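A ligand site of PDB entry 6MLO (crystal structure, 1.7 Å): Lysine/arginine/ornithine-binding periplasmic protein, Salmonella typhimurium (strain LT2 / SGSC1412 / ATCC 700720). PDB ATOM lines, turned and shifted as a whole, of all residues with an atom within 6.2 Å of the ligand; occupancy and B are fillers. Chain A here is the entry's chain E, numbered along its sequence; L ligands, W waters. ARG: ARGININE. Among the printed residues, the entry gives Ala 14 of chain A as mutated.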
ATOM      1  N   THR A  10       9.523   9.826 -11.965  1.00  0.00           N
ATOM      2  CA  THR A  10       9.930   8.568 -12.594  1.00  0.00           C
ATOM      3  C   THR A  10       8.938   8.239 -13.692  1.00  0.00           C
ATOM      4  O   THR A  10       7.799   8.701 -13.671  1.00  0.00           O
ATOM      5  CB  THR A  10      10.043   7.419 -11.558  1.00  0.00           C
ATOM      6  OG1 THR A  10      10.728   6.296 -12.137  1.00  0.00           O
ATOM      7  CG2 THR A  10       8.672   6.952 -11.054  1.00  0.00           C
ATOM      8  N   ASP A  11       9.392   7.470 -14.674  1.00  0.00           N
ATOM      9  CA  ASP A  11       8.530   6.952 -15.715  1.00  0.00           C
ATOM     10  C   ASP A  11       8.236   5.517 -15.347  1.00  0.00           C
ATOM     11  O   ASP A  11       9.086   4.801 -15.070  1.00  0.00           O
ATOM     12  CB  ASP A  11       9.195   7.094 -17.120  1.00  0.00           C
ATOM     13  CG  ASP A  11       8.830   5.971 -18.075  1.00  0.00           C
ATOM     14  OD1 ASP A  11       8.010   6.153 -18.873  1.00  0.00           O
ATOM     15  OD2 ASP A  11       9.278   4.897 -17.874  1.00  0.00           O
ATOM     16  N   THR A  12       7.001   5.103 -15.458  1.00  0.00           N
ATOM     17  CA  THR A  12       6.598   3.808 -14.909  1.00  0.00           C
ATOM     18  C   THR A  12       6.367   2.740 -15.979  1.00  0.00           C
ATOM     19  O   THR A  12       5.485   1.886 -15.842  1.00  0.00           O
ATOM     20  CB  THR A  12       5.326   3.975 -14.078  1.00  0.00           C
ATOM     21  OG1 THR A  12       4.324   4.590 -14.894  1.00  0.00           O
ATOM     22  CG2 THR A  12       5.605   4.874 -12.881  1.00  0.00           C
ATOM     23  N   THR A  13       7.171   2.769 -17.039  1.00  0.00           N
ATOM     24  CA  THR A  13       7.059   1.734 -18.075  1.00  0.00           C
ATOM     25  C   THR A  13       8.368   0.924 -18.143  1.00  0.00           C
ATOM     26  O   THR A  13       8.755   0.434 -19.204  1.00  0.00           O
ATOM     27  CB  THR A  13       6.701   2.335 -19.473  1.00  0.00           C
ATOM     28  OG1 THR A  13       7.716   3.266 -19.885  1.00  0.00           O
ATOM     29  CG2 THR A  13       5.372   3.061 -19.415  1.00  0.00           C
ATOM     30  N   ALA A  14       9.043   0.779 -16.993  1.00  0.00           N
ATOM     31  CA  ALA A  14      10.371   0.174 -16.967  1.00  0.00           C
ATOM     32  C   ALA A  14      10.560  -0.877 -15.867  1.00  0.00           C
ATOM     33  O   ALA A  14      11.550  -0.819 -15.127  1.00  0.00           O
ATOM     34  CB  ALA A  14      11.438   1.261 -16.830  1.00  0.00           C
ATOM     35  N   SER A  18      11.095   0.493 -12.542  1.00  0.00           N
ATOM     36  CA  SER A  18      10.019   1.399 -12.181  1.00  0.00           C
ATOM     37  C   SER A  18       8.770   1.120 -12.996  1.00  0.00           C
ATOM     38  O   SER A  18       8.809   1.166 -14.230  1.00  0.00           O
ATOM     39  CB  SER A  18      10.452   2.852 -12.362  1.00  0.00           C
ATOM     40  OG  SER A  18       9.408   3.741 -12.019  1.00  0.00           O
ATOM     41  N   ASP A  30      14.226   0.821  -8.688  1.00  0.00           N
ATOM     42  CA  ASP A  30      14.416   2.275  -8.551  1.00  0.00           C
ATOM     43  C   ASP A  30      13.620   2.810  -7.355  1.00  0.00           C
ATOM     44  O   ASP A  30      14.105   3.670  -6.598  1.00  0.00           O
ATOM     45  CB  ASP A  30      13.948   3.022  -9.806  1.00  0.00           C
ATOM     46  CG  ASP A  30      15.020   3.113 -10.890  1.00  0.00           C
ATOM     47  OD1 ASP A  30      16.182   2.720 -10.655  1.00  0.00           O
ATOM     48  OD2 ASP A  30      14.680   3.597 -11.992  1.00  0.00           O
ATOM     49  N   PHE A  52       8.934   9.704 -19.749  1.00  0.00           N
ATOM     50  CA  PHE A  52      10.380   9.812 -19.577  1.00  0.00           C
ATOM     51  C   PHE A  52      10.927  11.147 -20.076  1.00  0.00           C
ATOM     52  O   PHE A  52      11.787  11.767 -19.406  1.00  0.00           O
ATOM     53  CB  PHE A  52      11.099   8.641 -20.272  1.00  0.00           C
ATOM     54  CG  PHE A  52      12.573   8.622 -19.992  1.00  0.00           C
ATOM     55  CD1 PHE A  52      13.051   8.099 -18.799  1.00  0.00           C
ATOM     56  CD2 PHE A  52      13.479   9.186 -20.890  1.00  0.00           C
ATOM     57  CE1 PHE A  52      14.420   8.105 -18.517  1.00  0.00           C
ATOM     58  CE2 PHE A  52      14.842   9.195 -20.621  1.00  0.00           C
ATOM     59  CZ  PHE A  52      15.314   8.657 -19.430  1.00  0.00           C
ATOM     60  N   LEU A  55      10.926  14.304 -17.743  1.00  0.00           N
ATOM     61  CA  LEU A  55      11.603  14.264 -16.442  1.00  0.00           C
ATOM     62  C   LEU A  55      12.639  15.377 -16.270  1.00  0.00           C
ATOM     63  O   LEU A  55      12.600  16.137 -15.297  1.00  0.00           O
ATOM     64  CB  LEU A  55      12.269  12.899 -16.212  1.00  0.00           C
ATOM     65  CG  LEU A  55      11.298  11.721 -16.019  1.00  0.00           C
ATOM     66  CD1 LEU A  55      12.021  10.386 -16.039  1.00  0.00           C
ATOM     67  CD2 LEU A  55      10.547  11.901 -14.711  1.00  0.00           C
ATOM     68  N   SER A  69      14.954   6.966 -12.500  1.00  0.00           N
ATOM     69  CA  SER A  69      14.216   6.399 -13.613  1.00  0.00           C
ATOM     70  C   SER A  69      15.146   5.740 -14.639  1.00  0.00           C
ATOM     71  O   SER A  69      15.027   5.960 -15.781  1.00  0.00           O
ATOM     72  CB  SER A  69      13.387   7.482 -14.276  1.00  0.00           C
ATOM     73  OG  SER A  69      12.284   6.944 -14.943  1.00  0.00           O
ATOM     74  N   SER A  70      16.082   4.963 -14.138  1.00  0.00           N
ATOM     75  CA  SER A  70      17.131   4.386 -14.974  1.00  0.00           C
ATOM     76  C   SER A  70      17.796   5.460 -15.819  1.00  0.00           C
ATOM     77  O   SER A  70      18.126   5.229 -16.984  1.00  0.00           O
ATOM     78  CB  SER A  70      16.564   3.285 -15.889  1.00  0.00           C
ATOM     79  OG  SER A  70      16.101   2.182 -15.124  1.00  0.00           O
ATOM     80  N   LEU A  71      17.992   6.640 -15.223  1.00  0.00           N
ATOM     81  CA  LEU A  71      18.539   7.786 -15.953  1.00  0.00           C
ATOM     82  C   LEU A  71      20.044   7.685 -16.089  1.00  0.00           C
ATOM     83  O   LEU A  71      20.769   7.872 -15.118  1.00  0.00           O
ATOM     84  CB  LEU A  71      18.187   9.097 -15.234  1.00  0.00           C
ATOM     85  CG  LEU A  71      18.447  10.394 -16.002  1.00  0.00           C
ATOM     86  CD1 LEU A  71      17.407  10.560 -17.113  1.00  0.00           C
ATOM     87  CD2 LEU A  71      18.431  11.597 -15.070  1.00  0.00           C
ATOM     88  N   SER A  72      20.512   7.389 -17.296  1.00  0.00           N
ATOM     89  CA  SER A  72      21.941   7.231 -17.562  1.00  0.00           C
ATOM     90  C   SER A  72      22.742   8.516 -17.378  1.00  0.00           C
ATOM     91  O   SER A  72      22.340   9.604 -17.774  1.00  0.00           O
ATOM     92  CB  SER A  72      22.142   6.704 -18.986  1.00  0.00           C
ATOM     93  OG  SER A  72      21.656   5.380 -19.069  1.00  0.00           O
ATOM     94  N   ILE A  73      23.908   8.352 -16.752  1.00  0.00           N
ATOM     95  CA  ILE A  73      24.823   9.437 -16.468  1.00  0.00           C
ATOM     96  C   ILE A  73      25.647   9.673 -17.718  1.00  0.00           C
ATOM     97  O   ILE A  73      26.603   8.936 -17.980  1.00  0.00           O
ATOM     98  CB  ILE A  73      25.768   9.103 -15.268  1.00  0.00           C
ATOM     99  CG1 ILE A  73      24.940   8.768 -14.023  1.00  0.00           C
ATOM    100  CG2 ILE A  73      26.694  10.271 -14.972  1.00  0.00           C
ATOM    101  CD1 ILE A  73      25.746   8.109 -12.930  1.00  0.00           C
ATOM    102  N   THR A  74      25.257  10.658 -18.506  1.00  0.00           N
ATOM    103  CA  THR A  74      25.978  10.961 -19.742  1.00  0.00           C
ATOM    104  C   THR A  74      26.669  12.310 -19.677  1.00  0.00           C
ATOM    105  O   THR A  74      26.277  13.196 -18.913  1.00  0.00           O
ATOM    106  CB  THR A  74      25.043  10.954 -20.970  1.00  0.00           C
ATOM    107  OG1 THR A  74      24.154  12.079 -20.885  1.00  0.00           O
ATOM    108  CG2 THR A  74      24.239   9.670 -21.018  1.00  0.00           C
ATOM    109  N   ARG A  77      24.114  15.054 -20.599  1.00  0.00           N
ATOM    110  CA  ARG A  77      23.201  15.454 -19.532  1.00  0.00           C
ATOM    111  C   ARG A  77      23.893  16.221 -18.404  1.00  0.00           C
ATOM    112  O   ARG A  77      23.296  17.110 -17.771  1.00  0.00           O
ATOM    113  CB  ARG A  77      22.487  14.231 -18.965  1.00  0.00           C
ATOM    114  CG  ARG A  77      21.359  13.767 -19.860  1.00  0.00           C
ATOM    115  CD  ARG A  77      20.980  12.349 -19.501  1.00  0.00           C
ATOM    116  NE  ARG A  77      19.864  11.909 -20.330  1.00  0.00           N
ATOM    117  CZ  ARG A  77      19.377  10.673 -20.323  1.00  0.00           C
ATOM    118  NH1 ARG A  77      19.915   9.745 -19.529  1.00  0.00           N
ATOM    119  NH2 ARG A  77      18.361  10.363 -21.121  1.00  0.00           N
ATOM    120  N   ALA A  90      24.132   0.109 -16.741  1.00  0.00           N
ATOM    121  CA  ALA A  90      23.106  -0.103 -17.759  1.00  0.00           C
ATOM    122  C   ALA A  90      23.738  -0.141 -19.135  1.00  0.00           C
ATOM    123  O   ALA A  90      24.616   0.651 -19.455  1.00  0.00           O
ATOM    124  CB  ALA A  90      22.029   0.976 -17.693  1.00  0.00           C
ATOM    125  N   LEU A 117      12.499   5.034 -27.135  1.00  0.00           N
ATOM    126  CA  LEU A 117      11.789   5.901 -26.180  1.00  0.00           C
ATOM    127  C   LEU A 117      12.168   7.379 -26.332  1.00  0.00           C
ATOM    128  O   LEU A 117      13.347   7.734 -26.319  1.00  0.00           O
ATOM    129  CB  LEU A 117      12.085   5.449 -24.759  1.00  0.00           C
ATOM    130  CG  LEU A 117      11.533   6.322 -23.636  1.00  0.00           C
ATOM    131  CD1 LEU A 117      10.021   6.206 -23.602  1.00  0.00           C
ATOM    132  CD2 LEU A 117      12.170   5.872 -22.310  1.00  0.00           C
ATOM    133  N   GLY A 119      13.233  10.960 -25.699  1.00  0.00           N
ATOM    134  CA  GLY A 119      14.044  11.542 -24.650  1.00  0.00           C
ATOM    135  C   GLY A 119      15.163  10.654 -24.129  1.00  0.00           C
ATOM    136  O   GLY A 119      15.904  11.060 -23.240  1.00  0.00           O
ATOM    137  N   SER A 120      15.287   9.440 -24.673  1.00  0.00           N
ATOM    138  CA  SER A 120      16.272   8.472 -24.171  1.00  0.00           C
ATOM    139  C   SER A 120      17.622   8.564 -24.875  1.00  0.00           C
ATOM    140  O   SER A 120      17.734   9.174 -25.935  1.00  0.00           O
ATOM    141  CB  SER A 120      15.749   7.032 -24.314  1.00  0.00           C
ATOM    142  OG  SER A 120      15.666   6.663 -25.689  1.00  0.00           O
ATOM    143  N   THR A 121      18.633   7.962 -24.272  1.00  0.00           N
ATOM    144  CA  THR A 121      19.932   7.859 -24.912  1.00  0.00           C
ATOM    145  C   THR A 121      19.847   7.003 -26.181  1.00  0.00           C
ATOM    146  O   THR A 121      20.581   7.212 -27.143  1.00  0.00           O
ATOM    147  CB  THR A 121      20.973   7.231 -23.982  1.00  0.00           C
ATOM    148  OG1 THR A 121      20.463   5.983 -23.487  1.00  0.00           O
ATOM    149  CG2 THR A 121      21.269   8.164 -22.804  1.00  0.00           C
ATOM    150  N   GLN A 122      18.942   6.021 -26.145  1.00  0.00           N
ATOM    151  CA  GLN A 122      18.771   5.118 -27.276  1.00  0.00           C
ATOM    152  C   GLN A 122      18.200   5.896 -28.441  1.00  0.00           C
ATOM    153  O   GLN A 122      18.597   5.679 -29.588  1.00  0.00           O
ATOM    154  CB  GLN A 122      17.878   3.944 -26.891  1.00  0.00           C
ATOM    155  CG  GLN A 122      18.527   2.970 -25.919  1.00  0.00           C
ATOM    156  CD  GLN A 122      18.322   3.334 -24.455  1.00  0.00           C
ATOM    157  OE1 GLN A 122      17.512   4.208 -24.114  1.00  0.00           O
ATOM    158  NE2 GLN A 122      19.070   2.675 -23.592  1.00  0.00           N
ATOM    159  N   GLN A 143       7.573   3.284 -23.157  1.00  0.00           N
ATOM    160  CA  GLN A 143       8.090   2.008 -23.622  1.00  0.00           C
ATOM    161  C   GLN A 143       6.964   0.961 -23.771  1.00  0.00           C
ATOM    162  O   GLN A 143       7.128   0.012 -24.527  1.00  0.00           O
ATOM    163  CB  GLN A 143       9.205   1.500 -22.685  1.00  0.00           C
ATOM    164  CG  GLN A 143       9.964   0.249 -23.151  1.00  0.00           C
ATOM    165  CD  GLN A 143      11.062   0.495 -24.206  1.00  0.00           C
ATOM    166  OE1 GLN A 143      11.687   1.559 -24.257  1.00  0.00           O
ATOM    167  NE2 GLN A 143      11.303  -0.522 -25.029  1.00  0.00           N
ATOM    168  N   ASP A 161      17.165  -0.202 -22.747  1.00  0.00           N
ATOM    169  CA  ASP A 161      18.081  -0.693 -21.733  1.00  0.00           C
ATOM    170  C   ASP A 161      17.979  -2.217 -21.721  1.00  0.00           C
ATOM    171  O   ASP A 161      16.883  -2.784 -21.783  1.00  0.00           O
ATOM    172  CB  ASP A 161      17.789  -0.113 -20.336  1.00  0.00           C
ATOM    173  CG  ASP A 161      18.404   1.289 -20.107  1.00  0.00           C
ATOM    174  OD1 ASP A 161      19.255   1.784 -20.893  1.00  0.00           O
ATOM    175  OD2 ASP A 161      18.039   1.898 -19.066  1.00  0.00           O
ATOM    176  N   PHE A 191      25.725   6.487 -24.341  1.00  0.00           N
ATOM    177  CA  PHE A 191      25.004   5.706 -23.345  1.00  0.00           C
ATOM    178  C   PHE A 191      25.477   5.950 -21.925  1.00  0.00           C
ATOM    179  O   PHE A 191      24.793   5.569 -20.972  1.00  0.00           O
ATOM    180  CB  PHE A 191      25.089   4.227 -23.677  1.00  0.00           C
ATOM    181  CG  PHE A 191      24.471   3.879 -25.000  1.00  0.00           C
ATOM    182  CD1 PHE A 191      23.239   4.392 -25.344  1.00  0.00           C
ATOM    183  CD2 PHE A 191      25.129   3.063 -25.895  1.00  0.00           C
ATOM    184  CE1 PHE A 191      22.661   4.088 -26.559  1.00  0.00           C
ATOM    185  CE2 PHE A 191      24.561   2.762 -27.113  1.00  0.00           C
ATOM    186  CZ  PHE A 191      23.324   3.269 -27.441  1.00  0.00           C
ATOM    187  N   THR A 195      23.476   4.440 -14.291  1.00  0.00           N
ATOM    188  CA  THR A 195      22.418   5.393 -14.002  1.00  0.00           C
ATOM    189  C   THR A 195      22.645   6.072 -12.661  1.00  0.00           C
ATOM    190  O   THR A 195      23.434   5.590 -11.839  1.00  0.00           O
ATOM    191  CB  THR A 195      21.054   4.724 -13.974  1.00  0.00           C
ATOM    192  OG1 THR A 195      20.993   3.854 -12.831  1.00  0.00           O
ATOM    193  CG2 THR A 195      20.841   3.928 -15.245  1.00  0.00           C
HETATM  194  N   ARG L   1      18.894   4.611 -19.553  1.00  0.00           N
HETATM  195  CA  ARG L   1      18.244   5.248 -20.691  1.00  0.00           C
HETATM  196  C   ARG L   1      18.345   6.760 -20.572  1.00  0.00           C
HETATM  197  O   ARG L   1      18.812   7.270 -19.551  1.00  0.00           O
HETATM  198  CB  ARG L   1      16.779   4.821 -20.786  1.00  0.00           C
HETATM  199  CG  ARG L   1      16.039   4.938 -19.470  1.00  0.00           C
HETATM  200  CD  ARG L   1      14.549   4.660 -19.605  1.00  0.00           C
HETATM  201  NE  ARG L   1      13.880   4.743 -18.304  1.00  0.00           N
HETATM  202  CZ  ARG L   1      12.575   4.586 -18.096  1.00  0.00           C
HETATM  203  NH1 ARG L   1      11.756   4.317 -19.102  1.00  0.00           N
HETATM  204  NH2 ARG L   1      12.082   4.700 -16.871  1.00  0.00           N
HETATM  205  OXT ARG L   1      17.938   7.499 -21.491  1.00  0.00           O
HETATM  206  O   HOH W   1      12.542   2.531 -21.725  1.00  0.00           O
HETATM  207  O   HOH W   2      15.422   1.766 -21.777  1.00  0.00           O
HETATM  208  O   HOH W   3      13.472   3.051 -14.389  1.00  0.00           O
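Water W1 bridges OE1 of Gln 143 (2.8 Å) and NH1 of the ligand (3.3 Å).
Water W3 lies within hydrogen-bond range of OD2 of Asp 30 (2.7 Å), OG of Ser 70 (2.9 Å) and NH2 of the ligand (3.3 Å).
The side-chain carboxylate (OD1) of Asp 161 is in hydrogen-bond range of the side-chain amide nitrogen (NE2) of Gln 122 (2.8 Å).
OD2 of Asp 30 lies close to N of Ser 69, 3.4 Å away.
OG of Ser 69 is in hydrogen-bond range of OG1 of Thr 10, at 3.3 Å.
The backbone carbonyl oxygen (O) of Asp 11 lies within hydrogen-bond range of the side-chain hydroxyl (OG) of Ser 18, 3.2 Å away.
The backbone NH (N) of Arg 77 is in hydrogen-bond range of the side-chain hydroxyl (OG1) of Thr 74 (3.0 Å).
The side-chain carboxylate of Asp 11 lies within hydrogen-bond range of the side-chain hydroxyl of Thr 13 (3.0 Å).
The backbone carbonyl oxygen (O) of Gly 119 sits at hydrogen-bond distance from the guanidinium group (NH2) of Arg 77 (3.3 Å).
O of Leu 117 sits at hydrogen-bond distance from OG of Ser 120 (2.6 Å).
CB of Ala 14 touches NH2 of the ligand, 3.5 Å away.
Phe 52 touches the ligand (CE1 to NE, 3.4 Å).
CA of Leu 71 touches O of the ligand (3.6 Å).
CD2 of Leu 117 touches NH1 of the ligand, at 3.6 Å.
Ser 120 touches the ligand.
Gln 122 touches the ligand.
Hydrophobic or aromatic side chains that line the ligand: Ala 14, Phe 52 and Leu 117.
Within 4 Å of the ligand: Asp 11, Ala 14, Phe 52, Ser 69, Ser 70, Leu 71, Ser 72, Arg 77, Leu 117, Ser 120, Thr 121, Gln 122 and Asp 161.
The nearest printed residue that does not touch the ligand is Thr 13 (4.2 Å).
A nitrogen (N) of the ligand is in hydrogen-bond range of the backbone carbonyl oxygen of Ser 70 (2.8 Å).
A nitrogen (NH1) of the ligand is in salt-bridge range of the side-chain carboxylate (OD2) of Asp 11, at 2.8 Å.
The side-chain hydroxyl (OG) of Ser 72 sits at hydrogen-bond distance from a nitrogen (N) of the ligand, 2.9 Å away.
NE of the ligand sits at hydrogen-bond distance from O of Ser 69 (3.0 Å).
The backbone NH of Ser 72 is in hydrogen-bond range of an oxygen (O) of the ligand (2.8 Å).
The backbone carbonyl oxygen (O) of Asp 11 sits at hydrogen-bond distance from a nitrogen (NH2) of the ligand, 3.5 Å away.
The guanidinium group (NH1) of Arg 77 lies within salt-bridge range of an oxygen (O) of the ligand (2.7 Å).
OD2 of Asp 161 lies within salt-bridge range of N of the ligand, 2.9 Å away.
The side-chain hydroxyl (OG) of Ser 69 lies within hydrogen-bond range of a nitrogen (NH2) of the ligand (3.0 Å).
N of Thr 121 is in hydrogen-bond range of OXT of the ligand, 2.9 Å away.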
